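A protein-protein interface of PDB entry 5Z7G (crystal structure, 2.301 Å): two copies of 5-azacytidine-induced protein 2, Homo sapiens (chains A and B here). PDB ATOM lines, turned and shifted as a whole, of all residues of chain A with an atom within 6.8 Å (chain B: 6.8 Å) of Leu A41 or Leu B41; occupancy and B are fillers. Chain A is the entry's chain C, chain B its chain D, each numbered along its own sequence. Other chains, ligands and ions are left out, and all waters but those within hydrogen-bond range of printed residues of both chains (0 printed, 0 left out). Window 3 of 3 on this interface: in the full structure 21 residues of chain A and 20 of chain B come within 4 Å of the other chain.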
ATOM      1  N   ARG A  33      22.963   8.789  18.905  1.00  0.00           N
ATOM      2  CA  ARG A  33      23.240   8.799  20.340  1.00  0.00           C
ATOM      3  C   ARG A  33      23.608   7.409  20.833  1.00  0.00           C
ATOM      4  O   ARG A  33      24.543   7.248  21.630  1.00  0.00           O
ATOM      5  CB  ARG A  33      22.046   9.345  21.125  1.00  0.00           C
ATOM      6  CG  ARG A  33      22.187   9.169  22.649  1.00  0.00           C
ATOM      7  CD  ARG A  33      21.392  10.206  23.405  1.00  0.00           C
ATOM      8  NE  ARG A  33      21.686  10.281  24.839  1.00  0.00           N
ATOM      9  CZ  ARG A  33      22.574  11.119  25.382  1.00  0.00           C
ATOM     10  NH1 ARG A  33      23.295  11.941  24.622  1.00  0.00           N
ATOM     11  NH2 ARG A  33      22.757  11.132  26.692  1.00  0.00           N
ATOM     12  N   PHE A  36      27.130   6.776  20.069  1.00  0.00           N
ATOM     13  CA  PHE A  36      27.933   7.616  20.947  1.00  0.00           C
ATOM     14  C   PHE A  36      27.994   7.043  22.358  1.00  0.00           C
ATOM     15  O   PHE A  36      29.063   7.005  22.973  1.00  0.00           O
ATOM     16  CB  PHE A  36      27.352   9.031  20.939  1.00  0.00           C
ATOM     17  CG  PHE A  36      27.779   9.882  22.096  1.00  0.00           C
ATOM     18  CD1 PHE A  36      28.990  10.560  22.068  1.00  0.00           C
ATOM     19  CD2 PHE A  36      26.947  10.041  23.195  1.00  0.00           C
ATOM     20  CE1 PHE A  36      29.381  11.368  23.135  1.00  0.00           C
ATOM     21  CE2 PHE A  36      27.327  10.858  24.262  1.00  0.00           C
ATOM     22  CZ  PHE A  36      28.541  11.518  24.232  1.00  0.00           C
ATOM     23  N   LEU A  37      26.860   6.566  22.877  1.00  0.00           N
ATOM     24  CA  LEU A  37      26.853   5.987  24.214  1.00  0.00           C
ATOM     25  C   LEU A  37      27.572   4.649  24.237  1.00  0.00           C
ATOM     26  O   LEU A  37      28.339   4.358  25.164  1.00  0.00           O
ATOM     27  CB  LEU A  37      25.417   5.803  24.692  1.00  0.00           C
ATOM     28  CG  LEU A  37      24.701   7.108  24.960  1.00  0.00           C
ATOM     29  CD1 LEU A  37      23.322   6.799  25.483  1.00  0.00           C
ATOM     30  CD2 LEU A  37      25.512   7.949  25.955  1.00  0.00           C
ATOM     31  N   GLU A  38      27.305   3.807  23.241  1.00  0.00           N
ATOM     32  CA  GLU A  38      27.934   2.498  23.223  1.00  0.00           C
ATOM     33  C   GLU A  38      29.445   2.631  23.130  1.00  0.00           C
ATOM     34  O   GLU A  38      30.174   1.867  23.777  1.00  0.00           O
ATOM     35  CB  GLU A  38      27.360   1.671  22.078  1.00  0.00           C
ATOM     36  CG  GLU A  38      25.947   1.172  22.369  1.00  0.00           C
ATOM     37  CD  GLU A  38      25.306   0.455  21.177  1.00  0.00           C
ATOM     38  OE1 GLU A  38      25.813   0.610  20.058  1.00  0.00           O
ATOM     39  OE2 GLU A  38      24.308  -0.283  21.360  1.00  0.00           O
ATOM     40  N   GLU A  39      29.929   3.638  22.393  1.00  0.00           N
ATOM     41  CA  GLU A  39      31.369   3.868  22.289  1.00  0.00           C
ATOM     42  C   GLU A  39      32.017   4.031  23.658  1.00  0.00           C
ATOM     43  O   GLU A  39      33.190   3.690  23.834  1.00  0.00           O
ATOM     44  CB  GLU A  39      31.641   5.097  21.425  1.00  0.00           C
ATOM     45  CG  GLU A  39      33.046   5.163  20.857  1.00  0.00           C
ATOM     46  CD  GLU A  39      34.075   5.704  21.850  1.00  0.00           C
ATOM     47  OE1 GLU A  39      34.035   6.914  22.173  1.00  0.00           O
ATOM     48  OE2 GLU A  39      34.933   4.916  22.307  1.00  0.00           O
ATOM     49  N   LYS A  40      31.278   4.539  24.637  1.00  0.00           N
ATOM     50  CA  LYS A  40      31.804   4.616  25.992  1.00  0.00           C
ATOM     51  C   LYS A  40      31.769   3.284  26.717  1.00  0.00           C
ATOM     52  O   LYS A  40      32.367   3.171  27.791  1.00  0.00           O
ATOM     53  CB  LYS A  40      31.011   5.633  26.813  1.00  0.00           C
ATOM     54  CG  LYS A  40      30.966   7.025  26.182  1.00  0.00           C
ATOM     55  CD  LYS A  40      30.006   7.951  26.922  1.00  0.00           C
ATOM     56  CE  LYS A  40      30.056   9.358  26.335  1.00  0.00           C
ATOM     57  NZ  LYS A  40      31.302  10.092  26.725  1.00  0.00           N
ATOM     58  N   LEU A  41      31.087   2.279  26.173  1.00  0.00           N
ATOM     59  CA  LEU A  41      30.712   1.139  26.996  1.00  0.00           C
ATOM     60  C   LEU A  41      31.291  -0.191  26.543  1.00  0.00           C
ATOM     61  O   LEU A  41      31.743  -0.962  27.390  1.00  0.00           O
ATOM     62  CB  LEU A  41      29.177   1.030  27.082  1.00  0.00           C
ATOM     63  CG  LEU A  41      28.531   1.973  28.110  1.00  0.00           C
ATOM     64  CD1 LEU A  41      27.008   1.934  28.052  1.00  0.00           C
ATOM     65  CD2 LEU A  41      29.029   1.683  29.519  1.00  0.00           C
ATOM     66  N   ILE A  42      31.294  -0.508  25.246  1.00  0.00           N
ATOM     67  CA  ILE A  42      31.560  -1.902  24.909  1.00  0.00           C
ATOM     68  C   ILE A  42      32.753  -2.104  23.980  1.00  0.00           C
ATOM     69  O   ILE A  42      33.687  -2.839  24.325  1.00  0.00           O
ATOM     70  CB  ILE A  42      30.295  -2.578  24.352  1.00  0.00           C
ATOM     71  CG1 ILE A  42      29.666  -1.777  23.212  1.00  0.00           C
ATOM     72  CG2 ILE A  42      29.297  -2.781  25.487  1.00  0.00           C
ATOM     73  CD1 ILE A  42      28.659  -2.587  22.422  1.00  0.00           C
ATOM     74  N   ALA A  43      32.741  -1.493  22.805  1.00  0.00           N
ATOM     75  CA  ALA A  43      33.807  -1.773  21.848  1.00  0.00           C
ATOM     76  C   ALA A  43      33.833  -0.755  20.731  1.00  0.00           C
ATOM     77  O   ALA A  43      34.296  -1.072  19.633  1.00  0.00           O
ATOM     78  CB  ALA A  43      33.653  -3.174  21.270  1.00  0.00           C
ATOM     79  OXT ALA A  43      33.390   0.385  20.911  1.00  0.00           O
ATOM     80  N   PHE B  36      18.526   2.438  28.659  1.00  0.00           N
ATOM     81  CA  PHE B  36      19.343   1.345  29.172  1.00  0.00           C
ATOM     82  C   PHE B  36      20.824   1.712  29.148  1.00  0.00           C
ATOM     83  O   PHE B  36      21.547   1.460  30.121  1.00  0.00           O
ATOM     84  CB  PHE B  36      19.058   0.078  28.354  1.00  0.00           C
ATOM     85  CG  PHE B  36      20.094  -1.003  28.505  1.00  0.00           C
ATOM     86  CD1 PHE B  36      20.022  -1.915  29.559  1.00  0.00           C
ATOM     87  CD2 PHE B  36      21.117  -1.138  27.572  1.00  0.00           C
ATOM     88  CE1 PHE B  36      20.969  -2.939  29.692  1.00  0.00           C
ATOM     89  CE2 PHE B  36      22.067  -2.161  27.700  1.00  0.00           C
ATOM     90  CZ  PHE B  36      21.988  -3.062  28.762  1.00  0.00           C
ATOM     91  N   LEU B  37      21.287   2.332  28.058  1.00  0.00           N
ATOM     92  CA  LEU B  37      22.695   2.706  27.942  1.00  0.00           C
ATOM     93  C   LEU B  37      23.060   3.836  28.905  1.00  0.00           C
ATOM     94  O   LEU B  37      24.145   3.831  29.497  1.00  0.00           O
ATOM     95  CB  LEU B  37      23.007   3.112  26.504  1.00  0.00           C
ATOM     96  CG  LEU B  37      22.886   1.955  25.508  1.00  0.00           C
ATOM     97  CD1 LEU B  37      22.923   2.447  24.045  1.00  0.00           C
ATOM     98  CD2 LEU B  37      23.967   0.928  25.779  1.00  0.00           C
ATOM     99  N   GLU B  38      22.180   4.821  29.073  1.00  0.00           N
ATOM    100  CA  GLU B  38      22.454   5.859  30.060  1.00  0.00           C
ATOM    101  C   GLU B  38      22.467   5.269  31.463  1.00  0.00           C
ATOM    102  O   GLU B  38      23.302   5.641  32.297  1.00  0.00           O
ATOM    103  CB  GLU B  38      21.425   6.990  29.950  1.00  0.00           C
ATOM    104  CG  GLU B  38      21.503   7.787  28.654  1.00  0.00           C
ATOM    105  CD  GLU B  38      20.258   8.636  28.397  1.00  0.00           C
ATOM    106  OE1 GLU B  38      19.196   8.357  28.994  1.00  0.00           O
ATOM    107  OE2 GLU B  38      20.336   9.585  27.586  1.00  0.00           O
ATOM    108  N   GLU B  39      21.558   4.329  31.734  1.00  0.00           N
ATOM    109  CA  GLU B  39      21.509   3.699  33.047  1.00  0.00           C
ATOM    110  C   GLU B  39      22.770   2.897  33.321  1.00  0.00           C
ATOM    111  O   GLU B  39      23.225   2.829  34.465  1.00  0.00           O
ATOM    112  CB  GLU B  39      20.273   2.807  33.151  1.00  0.00           C
ATOM    113  CG  GLU B  39      20.121   2.090  34.474  1.00  0.00           C
ATOM    114  CD  GLU B  39      18.715   1.556  34.678  1.00  0.00           C
ATOM    115  OE1 GLU B  39      18.514   0.719  35.584  1.00  0.00           O
ATOM    116  OE2 GLU B  39      17.808   1.974  33.926  1.00  0.00           O
ATOM    117  N   LYS B  40      23.360   2.303  32.284  1.00  0.00           N
ATOM    118  CA  LYS B  40      24.590   1.553  32.482  1.00  0.00           C
ATOM    119  C   LYS B  40      25.721   2.451  32.933  1.00  0.00           C
ATOM    120  O   LYS B  40      26.560   2.022  33.728  1.00  0.00           O
ATOM    121  CB  LYS B  40      24.994   0.827  31.201  1.00  0.00           C
ATOM    122  CG  LYS B  40      24.385  -0.566  31.056  1.00  0.00           C
ATOM    123  CD  LYS B  40      25.286  -1.633  31.660  1.00  0.00           C
ATOM    124  CE  LYS B  40      24.537  -2.943  31.789  1.00  0.00           C
ATOM    125  NZ  LYS B  40      23.118  -2.681  32.124  1.00  0.00           N
ATOM    126  N   LEU B  41      25.756   3.697  32.454  1.00  0.00           N
ATOM    127  CA  LEU B  41      26.861   4.592  32.772  1.00  0.00           C
ATOM    128  C   LEU B  41      26.801   5.169  34.181  1.00  0.00           C
ATOM    129  O   LEU B  41      27.841   5.584  34.701  1.00  0.00           O
ATOM    130  CB  LEU B  41      26.916   5.749  31.779  1.00  0.00           C
ATOM    131  CG  LEU B  41      27.284   5.397  30.349  1.00  0.00           C
ATOM    132  CD1 LEU B  41      26.452   6.235  29.428  1.00  0.00           C
ATOM    133  CD2 LEU B  41      28.767   5.628  30.110  1.00  0.00           C
ATOM    134  N   ILE B  42      25.622   5.222  34.808  1.00  0.00           N
ATOM    135  CA  ILE B  42      25.542   5.863  36.118  1.00  0.00           C
ATOM    136  C   ILE B  42      26.113   4.955  37.196  1.00  0.00           C
ATOM    137  O   ILE B  42      26.673   5.437  38.187  1.00  0.00           O
ATOM    138  CB  ILE B  42      24.097   6.303  36.440  1.00  0.00           C
ATOM    139  CG1 ILE B  42      23.198   5.134  36.825  1.00  0.00           C
ATOM    140  CG2 ILE B  42      23.480   7.003  35.260  1.00  0.00           C
ATOM    141  CD1 ILE B  42      21.717   5.512  36.884  1.00  0.00           C
ATOM    142  N   ALA B  43      26.013   3.640  37.013  1.00  0.00           N
ATOM    143  CA  ALA B  43      26.513   2.678  37.988  1.00  0.00           C
ATOM    144  C   ALA B  43      28.039   2.634  37.985  1.00  0.00           C
ATOM    145  O   ALA B  43      28.688   3.169  37.084  1.00  0.00           O
ATOM    146  CB  ALA B  43      25.941   1.294  37.706  1.00  0.00           C
ATOM    147  OXT ALA B  43      28.658   2.067  38.887  1.00  0.00           O
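The guanidinium group (NH2) of Arg A33 lies within salt-bridge range of the side-chain carboxylate (OE2) of Glu B38 (3.0 Å).
Leu A37 touches Leu B37 (CD1 to CB, 3.8 Å).
Leu A37 touches Glu B38 (CD1 to CG, 3.8 Å).
CD2 of Leu A37 touches CD1 of Leu B41 (3.99 Å).
Leu B37 touches Glu A38.
Lys A40 touches Leu B41.
Leu A41 touches Leu B37 (CD1 to O, 3.7 Å).
Lys B40 touches Leu A41.
Leu A41 touches Leu B41.
Printed residues of chain B within 4 Å of Lys A40: Leu B41.
Of the printed residues of chain B, Leu A41 touches Leu B37 (3.7 Å), Lys B40 (3.9 Å) and Leu B41 (3.998 Å).
Printed residues of chain A within 4 Å of Glu B38: Arg A33 and Leu A37.
Of the printed residues of chain A, Leu B41 touches Leu A37 (3.99 Å), Lys A40 (3.99 Å) and Leu A41 (3.998 Å).
The nearest printed residue of chain B that does not touch Leu A41 is Glu B38 (5.7 Å).
The nearest printed residue of chain A that does not touch Leu B41 is Glu A38 (6.7 Å).
Of the 8 printed residues of chain B, 4 touch a printed residue of chain A.
Hydrophobic or aromatic side chains of chain B that line the printed part of chain A: Leu B37 and Leu B41.
Among the printed residues, Asp or Glu carboxylates within 4 Å of a Lys or Arg side-chain nitrogen of the other chain: Arg A33 with Glu B38 (3.0 Å).
Leu A37 touches its own counterpart, Leu B37.
Leu A37 touches Leu B41, and with the chains exchanged Leu A41 touches Leu B37.
Lys A40 touches Leu B41, and with the chains exchanged Leu A41 touches Lys B40.
Leu B41 touches its own counterpart, Leu A41.
Positions printed for both chains: 36, 37, 38, 39, 40, 41, 42 and 43.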
